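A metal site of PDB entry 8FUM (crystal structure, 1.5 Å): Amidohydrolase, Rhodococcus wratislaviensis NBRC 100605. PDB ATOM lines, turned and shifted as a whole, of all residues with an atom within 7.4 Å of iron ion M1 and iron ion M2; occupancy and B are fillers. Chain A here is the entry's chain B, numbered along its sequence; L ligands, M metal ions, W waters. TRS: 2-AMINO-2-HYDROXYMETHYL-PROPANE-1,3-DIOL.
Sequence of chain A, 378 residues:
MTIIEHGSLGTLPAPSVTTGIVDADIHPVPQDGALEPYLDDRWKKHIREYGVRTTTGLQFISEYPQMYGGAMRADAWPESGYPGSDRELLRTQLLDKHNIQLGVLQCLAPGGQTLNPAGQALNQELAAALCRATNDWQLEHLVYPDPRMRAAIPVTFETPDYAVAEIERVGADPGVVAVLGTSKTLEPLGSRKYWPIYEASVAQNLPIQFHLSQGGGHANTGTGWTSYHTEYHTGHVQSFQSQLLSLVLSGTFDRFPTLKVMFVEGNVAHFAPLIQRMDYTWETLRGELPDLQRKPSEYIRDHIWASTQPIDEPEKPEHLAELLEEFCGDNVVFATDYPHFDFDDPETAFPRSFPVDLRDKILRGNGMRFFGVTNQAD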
ATOM      1  N   ASP A  25      14.848  -6.606 -10.722  1.00  0.00           N
ATOM      2  CA  ASP A  25      14.285  -7.157  -9.470  1.00  0.00           C
ATOM      3  C   ASP A  25      15.249  -6.883  -8.308  1.00  0.00           C
ATOM      4  O   ASP A  25      16.229  -7.617  -8.123  1.00  0.00           O
ATOM      5  CB  ASP A  25      13.968  -8.641  -9.596  1.00  0.00           C
ATOM      6  CG  ASP A  25      13.142  -9.172  -8.428  1.00  0.00           C
ATOM      7  OD1 ASP A  25      12.370  -8.381  -7.834  1.00  0.00           O
ATOM      8  OD2 ASP A  25      13.229 -10.377  -8.122  1.00  0.00           O
ATOM      9  N   ILE A  26      14.913  -5.866  -7.515  1.00  0.00           N
ATOM     10  CA  ILE A  26      15.618  -5.502  -6.297  1.00  0.00           C
ATOM     11  C   ILE A  26      14.594  -5.446  -5.177  1.00  0.00           C
ATOM     12  O   ILE A  26      13.494  -4.933  -5.376  1.00  0.00           O
ATOM     13  CB  ILE A  26      16.263  -4.103  -6.474  1.00  0.00           C
ATOM     14  CG1 ILE A  26      17.260  -4.147  -7.626  1.00  0.00           C
ATOM     15  CG2 ILE A  26      16.919  -3.641  -5.167  1.00  0.00           C
ATOM     16  CD1 ILE A  26      17.675  -2.734  -8.086  1.00  0.00           C
ATOM     17  N   HIS A  27      14.969  -5.917  -3.989  1.00  0.00           N
ATOM     18  CA  HIS A  27      14.030  -6.027  -2.866  1.00  0.00           C
ATOM     19  C   HIS A  27      14.431  -5.145  -1.699  1.00  0.00           C
ATOM     20  O   HIS A  27      15.163  -5.581  -0.809  1.00  0.00           O
ATOM     21  CB  HIS A  27      13.905  -7.485  -2.425  1.00  0.00           C
ATOM     22  CG  HIS A  27      13.389  -8.358  -3.514  1.00  0.00           C
ATOM     23  ND1 HIS A  27      12.191  -8.091  -4.154  1.00  0.00           N
ATOM     24  CD2 HIS A  27      13.895  -9.456  -4.119  1.00  0.00           C
ATOM     25  CE1 HIS A  27      11.984  -8.985  -5.092  1.00  0.00           C
ATOM     26  NE2 HIS A  27      13.012  -9.819  -5.111  1.00  0.00           N
ATOM     27  N   ALA A  71      17.027 -16.642   3.658  1.00  0.00           N
ATOM     28  CA  ALA A  71      17.225 -16.638   2.220  1.00  0.00           C
ATOM     29  C   ALA A  71      17.940 -15.379   1.739  1.00  0.00           C
ATOM     30  O   ALA A  71      17.797 -14.990   0.585  1.00  0.00           O
ATOM     31  CB  ALA A  71      15.906 -16.845   1.456  1.00  0.00           C
ATOM     32  N   GLN A 106      10.941  -3.997  -6.112  1.00  0.00           N
ATOM     33  CA  GLN A 106       9.795  -4.875  -5.898  1.00  0.00           C
ATOM     34  C   GLN A 106       9.731  -5.140  -4.396  1.00  0.00           C
ATOM     35  O   GLN A 106      10.434  -6.003  -3.871  1.00  0.00           O
ATOM     36  CB  GLN A 106       9.930  -6.141  -6.713  1.00  0.00           C
ATOM     37  CG  GLN A 106      10.114  -5.848  -8.190  1.00  0.00           C
ATOM     38  CD  GLN A 106       9.891  -7.029  -9.091  1.00  0.00           C
ATOM     39  OE1 GLN A 106       9.207  -7.999  -8.719  1.00  0.00           O
ATOM     40  NE2 GLN A 106      10.438  -6.965 -10.288  1.00  0.00           N
ATOM     41  N   LEU A 108       8.416  -6.696  -1.328  1.00  0.00           N
ATOM     42  CA  LEU A 108       7.690  -7.935  -1.095  1.00  0.00           C
ATOM     43  C   LEU A 108       7.169  -8.090   0.325  1.00  0.00           C
ATOM     44  O   LEU A 108       6.605  -9.138   0.631  1.00  0.00           O
ATOM     45  CB  LEU A 108       8.606  -9.128  -1.365  1.00  0.00           C
ATOM     46  CG  LEU A 108       9.251  -9.252  -2.748  1.00  0.00           C
ATOM     47  CD1 LEU A 108      10.204 -10.443  -2.700  1.00  0.00           C
ATOM     48  CD2 LEU A 108       8.161  -9.398  -3.810  1.00  0.00           C
ATOM     49  N   THR A 114      11.198 -11.422   4.333  1.00  0.00           N
ATOM     50  CA  THR A 114      11.638 -11.703   2.970  1.00  0.00           C
ATOM     51  C   THR A 114      10.514 -11.739   1.946  1.00  0.00           C
ATOM     52  O   THR A 114      10.662 -11.182   0.854  1.00  0.00           O
ATOM     53  CB  THR A 114      12.392 -13.026   2.969  1.00  0.00           C
ATOM     54  OG1 THR A 114      13.568 -12.911   3.797  1.00  0.00           O
ATOM     55  CG2 THR A 114      12.776 -13.418   1.556  1.00  0.00           C
ATOM     56  N   LEU A 115       9.389 -12.389   2.254  1.00  0.00           N
ATOM     57  CA  LEU A 115       8.332 -12.565   1.249  1.00  0.00           C
ATOM     58  C   LEU A 115       7.000 -12.666   2.002  1.00  0.00           C
ATOM     59  O   LEU A 115       6.633 -13.746   2.461  1.00  0.00           O
ATOM     60  CB  LEU A 115       8.592 -13.804   0.409  1.00  0.00           C
ATOM     61  CG  LEU A 115       7.578 -14.229  -0.646  1.00  0.00           C
ATOM     62  CD1 LEU A 115       7.354 -13.180  -1.718  1.00  0.00           C
ATOM     63  CD2 LEU A 115       7.997 -15.555  -1.291  1.00  0.00           C
ATOM     64  N   HIS A 211       5.906 -11.069  -9.756  1.00  0.00           N
ATOM     65  CA  HIS A 211       7.020 -11.652  -9.021  1.00  0.00           C
ATOM     66  C   HIS A 211       6.588 -12.924  -8.312  1.00  0.00           C
ATOM     67  O   HIS A 211       5.465 -13.026  -7.805  1.00  0.00           O
ATOM     68  CB  HIS A 211       7.559 -10.667  -7.983  1.00  0.00           C
ATOM     69  CG  HIS A 211       8.831 -11.111  -7.325  1.00  0.00           C
ATOM     70  ND1 HIS A 211       8.858 -12.042  -6.307  1.00  0.00           N
ATOM     71  CD2 HIS A 211      10.115 -10.749  -7.535  1.00  0.00           C
ATOM     72  CE1 HIS A 211      10.102 -12.224  -5.922  1.00  0.00           C
ATOM     73  NE2 HIS A 211      10.895 -11.464  -6.655  1.00  0.00           N
ATOM     74  N   LEU A 212       7.500 -13.899  -8.287  1.00  0.00           N
ATOM     75  CA  LEU A 212       7.318 -15.101  -7.482  1.00  0.00           C
ATOM     76  C   LEU A 212       6.631 -14.809  -6.157  1.00  0.00           C
ATOM     77  O   LEU A 212       6.971 -13.849  -5.451  1.00  0.00           O
ATOM     78  CB  LEU A 212       8.711 -15.705  -7.271  1.00  0.00           C
ATOM     79  CG  LEU A 212       9.110 -16.750  -6.248  1.00  0.00           C
ATOM     80  CD1 LEU A 212      10.504 -17.178  -6.668  1.00  0.00           C
ATOM     81  CD2 LEU A 212       9.120 -16.215  -4.826  1.00  0.00           C
ATOM     82  N   HIS A 233      11.029 -24.519  -3.796  1.00  0.00           N
ATOM     83  CA  HIS A 233      11.716 -23.477  -4.538  1.00  0.00           C
ATOM     84  C   HIS A 233      11.701 -23.777  -6.026  1.00  0.00           C
ATOM     85  O   HIS A 233      11.321 -22.919  -6.847  1.00  0.00           O
ATOM     86  CB  HIS A 233      13.114 -23.319  -3.948  1.00  0.00           C
ATOM     87  CG  HIS A 233      13.806 -22.058  -4.380  1.00  0.00           C
ATOM     88  ND1 HIS A 233      14.946 -21.604  -3.759  1.00  0.00           N
ATOM     89  CD2 HIS A 233      13.512 -21.150  -5.340  1.00  0.00           C
ATOM     90  CE1 HIS A 233      15.346 -20.482  -4.345  1.00  0.00           C
ATOM     91  NE2 HIS A 233      14.497 -20.192  -5.318  1.00  0.00           N
ATOM     92  N   VAL A 264       8.749 -12.491 -13.337  1.00  0.00           N
ATOM     93  CA  VAL A 264       9.955 -12.194 -12.572  1.00  0.00           C
ATOM     94  C   VAL A 264      10.230 -13.318 -11.586  1.00  0.00           C
ATOM     95  O   VAL A 264       9.415 -13.607 -10.700  1.00  0.00           O
ATOM     96  CB  VAL A 264       9.834 -10.849 -11.848  1.00  0.00           C
ATOM     97  CG1 VAL A 264      11.057 -10.600 -10.966  1.00  0.00           C
ATOM     98  CG2 VAL A 264       9.602  -9.718 -12.861  1.00  0.00           C
ATOM     99  N   GLU A 265      11.384 -13.962 -11.735  1.00  0.00           N
ATOM    100  CA  GLU A 265      11.864 -14.999 -10.844  1.00  0.00           C
ATOM    101  C   GLU A 265      11.073 -16.293 -11.008  1.00  0.00           C
ATOM    102  O   GLU A 265      11.005 -17.114 -10.084  1.00  0.00           O
ATOM    103  CB  GLU A 265      11.935 -14.544  -9.385  1.00  0.00           C
ATOM    104  CG  GLU A 265      13.013 -15.241  -8.576  1.00  0.00           C
ATOM    105  CD  GLU A 265      13.412 -14.453  -7.365  1.00  0.00           C
ATOM    106  OE1 GLU A 265      13.273 -13.193  -7.439  1.00  0.00           O
ATOM    107  OE2 GLU A 265      13.850 -15.057  -6.352  1.00  0.00           O
ATOM    108  N   GLN A 309      17.070 -13.988 -13.258  1.00  0.00           N
ATOM    109  CA  GLN A 309      17.521 -14.579 -12.009  1.00  0.00           C
ATOM    110  C   GLN A 309      16.454 -15.536 -11.469  1.00  0.00           C
ATOM    111  O   GLN A 309      15.258 -15.258 -11.579  1.00  0.00           O
ATOM    112  CB  GLN A 309      17.811 -13.464 -10.986  1.00  0.00           C
ATOM    113  CG  GLN A 309      18.338 -13.880  -9.625  1.00  0.00           C
ATOM    114  CD  GLN A 309      17.287 -14.434  -8.703  1.00  0.00           C
ATOM    115  OE1 GLN A 309      16.102 -14.195  -8.864  1.00  0.00           O
ATOM    116  NE2 GLN A 309      17.746 -15.141  -7.687  1.00  0.00           N
ATOM    117  N   PRO A 310      16.838 -16.668 -10.884  1.00  0.00           N
ATOM    118  CA  PRO A 310      18.194 -17.216 -10.800  1.00  0.00           C
ATOM    119  C   PRO A 310      18.518 -17.883 -12.123  1.00  0.00           C
ATOM    120  O   PRO A 310      17.760 -18.721 -12.623  1.00  0.00           O
ATOM    121  CB  PRO A 310      18.087 -18.219  -9.677  1.00  0.00           C
ATOM    122  CG  PRO A 310      16.651 -18.707  -9.730  1.00  0.00           C
ATOM    123  CD  PRO A 310      15.849 -17.514 -10.178  1.00  0.00           C
ATOM    124  N   ALA A 335      18.177  -9.401 -14.004  1.00  0.00           N
ATOM    125  CA  ALA A 335      17.894  -9.033 -12.631  1.00  0.00           C
ATOM    126  C   ALA A 335      18.962  -9.650 -11.728  1.00  0.00           C
ATOM    127  O   ALA A 335      19.475 -10.740 -12.003  1.00  0.00           O
ATOM    128  CB  ALA A 335      16.519  -9.575 -12.204  1.00  0.00           C
ATOM    129  N   THR A 336      19.218  -8.977 -10.608  1.00  0.00           N
ATOM    130  CA  THR A 336      20.103  -9.515  -9.585  1.00  0.00           C
ATOM    131  C   THR A 336      19.383 -10.258  -8.470  1.00  0.00           C
ATOM    132  O   THR A 336      19.937 -11.213  -7.932  1.00  0.00           O
ATOM    133  CB  THR A 336      20.968  -8.435  -8.895  1.00  0.00           C
ATOM    134  OG1 THR A 336      20.150  -7.548  -8.125  1.00  0.00           O
ATOM    135  CG2 THR A 336      21.831  -7.672  -9.890  1.00  0.00           C
ATOM    136  N   ASP A 337      18.175  -9.828  -8.110  1.00  0.00           N
ATOM    137  CA  ASP A 337      17.475 -10.282  -6.918  1.00  0.00           C
ATOM    138  C   ASP A 337      18.158  -9.866  -5.616  1.00  0.00           C
ATOM    139  O   ASP A 337      17.966 -10.507  -4.578  1.00  0.00           O
ATOM    140  CB  ASP A 337      17.247 -11.792  -6.927  1.00  0.00           C
ATOM    141  CG  ASP A 337      16.028 -12.193  -6.140  1.00  0.00           C
ATOM    142  OD1 ASP A 337      15.068 -11.387  -6.120  1.00  0.00           O
ATOM    143  OD2 ASP A 337      16.031 -13.303  -5.553  1.00  0.00           O
ATOM    144  N   TYR A 338      18.963  -8.811  -5.635  1.00  0.00           N
ATOM    145  CA  TYR A 338      19.555  -8.332  -4.399  1.00  0.00           C
ATOM    146  C   TYR A 338      18.456  -8.054  -3.377  1.00  0.00           C
ATOM    147  O   TYR A 338      17.470  -7.394  -3.715  1.00  0.00           O
ATOM    148  CB  TYR A 338      20.291  -7.024  -4.693  1.00  0.00           C
ATOM    149  CG  TYR A 338      20.974  -6.449  -3.473  1.00  0.00           C
ATOM    150  CD1 TYR A 338      22.263  -6.850  -3.130  1.00  0.00           C
ATOM    151  CD2 TYR A 338      20.326  -5.528  -2.656  1.00  0.00           C
ATOM    152  CE1 TYR A 338      22.884  -6.353  -1.988  1.00  0.00           C
ATOM    153  CE2 TYR A 338      20.941  -5.012  -1.539  1.00  0.00           C
ATOM    154  CZ  TYR A 338      22.218  -5.434  -1.200  1.00  0.00           C
ATOM    155  OH  TYR A 338      22.823  -4.918  -0.084  1.00  0.00           O
ATOM    156  N   PRO A 339      18.618  -8.461  -2.096  1.00  0.00           N
ATOM    157  CA  PRO A 339      19.775  -9.125  -1.489  1.00  0.00           C
ATOM    158  C   PRO A 339      19.599 -10.611  -1.212  1.00  0.00           C
ATOM    159  O   PRO A 339      20.178 -11.122  -0.248  1.00  0.00           O
ATOM    160  CB  PRO A 339      19.921  -8.367  -0.160  1.00  0.00           C
ATOM    161  CG  PRO A 339      18.499  -7.967   0.199  1.00  0.00           C
ATOM    162  CD  PRO A 339      17.648  -8.080  -1.069  1.00  0.00           C
ATOM    163  N   HIS A 340      18.836 -11.320  -2.042  1.00  0.00           N
ATOM    164  CA  HIS A 340      18.555 -12.714  -1.749  1.00  0.00           C
ATOM    165  C   HIS A 340      19.780 -13.592  -2.022  1.00  0.00           C
ATOM    166  O   HIS A 340      20.682 -13.228  -2.779  1.00  0.00           O
ATOM    167  CB  HIS A 340      17.346 -13.204  -2.555  1.00  0.00           C
ATOM    168  CG  HIS A 340      16.073 -12.543  -2.136  1.00  0.00           C
ATOM    169  ND1 HIS A 340      14.851 -12.850  -2.699  1.00  0.00           N
ATOM    170  CD2 HIS A 340      15.831 -11.598  -1.197  1.00  0.00           C
ATOM    171  CE1 HIS A 340      13.916 -12.106  -2.136  1.00  0.00           C
ATOM    172  NE2 HIS A 340      14.473 -11.360  -1.196  1.00  0.00           N
ATOM    173  N   PHE A 341      19.784 -14.766  -1.382  1.00  0.00           N
ATOM    174  CA  PHE A 341      20.978 -15.608  -1.346  1.00  0.00           C
ATOM    175  C   PHE A 341      21.394 -16.070  -2.732  1.00  0.00           C
ATOM    176  O   PHE A 341      22.592 -16.295  -2.982  1.00  0.00           O
ATOM    177  CB  PHE A 341      20.765 -16.822  -0.405  1.00  0.00           C
ATOM    178  CG  PHE A 341      20.051 -17.989  -1.050  1.00  0.00           C
ATOM    179  CD1 PHE A 341      18.662 -18.027  -1.093  1.00  0.00           C
ATOM    180  CD2 PHE A 341      20.769 -19.036  -1.614  1.00  0.00           C
ATOM    181  CE1 PHE A 341      18.012 -19.107  -1.691  1.00  0.00           C
ATOM    182  CE2 PHE A 341      20.129 -20.100  -2.200  1.00  0.00           C
ATOM    183  CZ  PHE A 341      18.750 -20.139  -2.241  1.00  0.00           C
ATOM    184  N   ASP A 342      20.439 -16.269  -3.641  1.00  0.00           N
ATOM    185  CA  ASP A 342      20.735 -16.701  -4.996  1.00  0.00           C
ATOM    186  C   ASP A 342      20.876 -15.529  -5.978  1.00  0.00           C
ATOM    187  O   ASP A 342      20.681 -15.691  -7.191  1.00  0.00           O
ATOM    188  CB  ASP A 342      19.744 -17.780  -5.479  1.00  0.00           C
ATOM    189  CG  ASP A 342      18.263 -17.350  -5.379  1.00  0.00           C
ATOM    190  OD1 ASP A 342      17.971 -16.273  -4.824  1.00  0.00           O
ATOM    191  OD2 ASP A 342      17.401 -18.115  -5.890  1.00  0.00           O
ATOM    192  N   PHE A 343      21.226 -14.365  -5.433  1.00  0.00           N
ATOM    193  CA  PHE A 343      21.671 -13.209  -6.187  1.00  0.00           C
ATOM    194  C   PHE A 343      22.542 -13.605  -7.376  1.00  0.00           C
ATOM    195  O   PHE A 343      23.438 -14.449  -7.258  1.00  0.00           O
ATOM    196  CB  PHE A 343      22.505 -12.370  -5.216  1.00  0.00           C
ATOM    197  CG  PHE A 343      23.243 -11.215  -5.843  1.00  0.00           C
ATOM    198  CD1 PHE A 343      22.645  -9.973  -5.993  1.00  0.00           C
ATOM    199  CD2 PHE A 343      24.548 -11.375  -6.255  1.00  0.00           C
ATOM    200  CE1 PHE A 343      23.341  -8.915  -6.572  1.00  0.00           C
ATOM    201  CE2 PHE A 343      25.232 -10.335  -6.825  1.00  0.00           C
ATOM    202  CZ  PHE A 343      24.633  -9.102  -6.980  1.00  0.00           C
HETATM  203  C   TRS L   1      13.584 -16.530  -2.833  1.00  0.00           C
HETATM  204  C1  TRS L   1      14.986 -16.856  -3.377  1.00  0.00           C
HETATM  205  C2  TRS L   1      13.670 -15.931  -1.417  1.00  0.00           C
HETATM  206  C3  TRS L   1      12.753 -17.812  -2.857  1.00  0.00           C
HETATM  207  N   TRS L   1      12.936 -15.534  -3.677  1.00  0.00           N
HETATM  208  O1  TRS L   1      15.595 -15.683  -3.872  1.00  0.00           O
HETATM  209  O2  TRS L   1      12.382 -15.476  -1.037  1.00  0.00           O
HETATM  210  O3  TRS L   1      13.364 -18.776  -2.020  1.00  0.00           O
HETATM  211 FE    FE M   1      14.317 -14.011  -4.547  1.00  0.00          FE
HETATM  212 FE    FE M   2      13.044 -11.496  -6.362  1.00  0.00          FE
HETATM  213  O   HOH W   1      12.781 -12.663  -4.821  1.00  0.00           O
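Within 4 Å of iron ion M1: Glu 265, Asp 337 and His 340.
The nearest printed residue that does not touch iron ion M1 is Asp 342 (4.3 Å).
Iron ion M1 is bound by water W1 (2.1 Å), the side-chain carboxylate (OD2) of Asp 337 (2.1 Å), the side-chain carboxylate (OE2) of Glu 265 (2.1 Å), an oxygen (O1) of the ligand (2.2 Å), a nitrogen (N) of the ligand (2.2 Å) and a ring nitrogen (ND1) of His 340 (2.2 Å).
OE1 of Glu 265 lies close to OE1 of Gln 309 (3.3 Å).
OD2 of Asp 337 lies close to NE2 of Gln 309, at 3.3 Å.
ND1 of His 27 lies within hydrogen-bond range of O of Gln 106 (2.7 Å).
The backbone NH (N) of His 27 is in hydrogen-bond range of the backbone carbonyl oxygen (O) of Tyr 338 (2.9 Å).
The side-chain amide oxygen (OE1) of Gln 106 lies close to the side-chain carboxylate (OD1) of Asp 25 (3.3 Å).
Iron ion M2 is bound by water W1 (2.0 Å), OE1 of Glu 265 (2.0 Å), OD1 of Asp 337 (2.0 Å), NE2 of His 27 (2.1 Å), OD2 of Asp 25 (2.1 Å) and NE2 of His 211 (2.2 Å).
Iron ion M2 has six donor atoms within binding distance.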
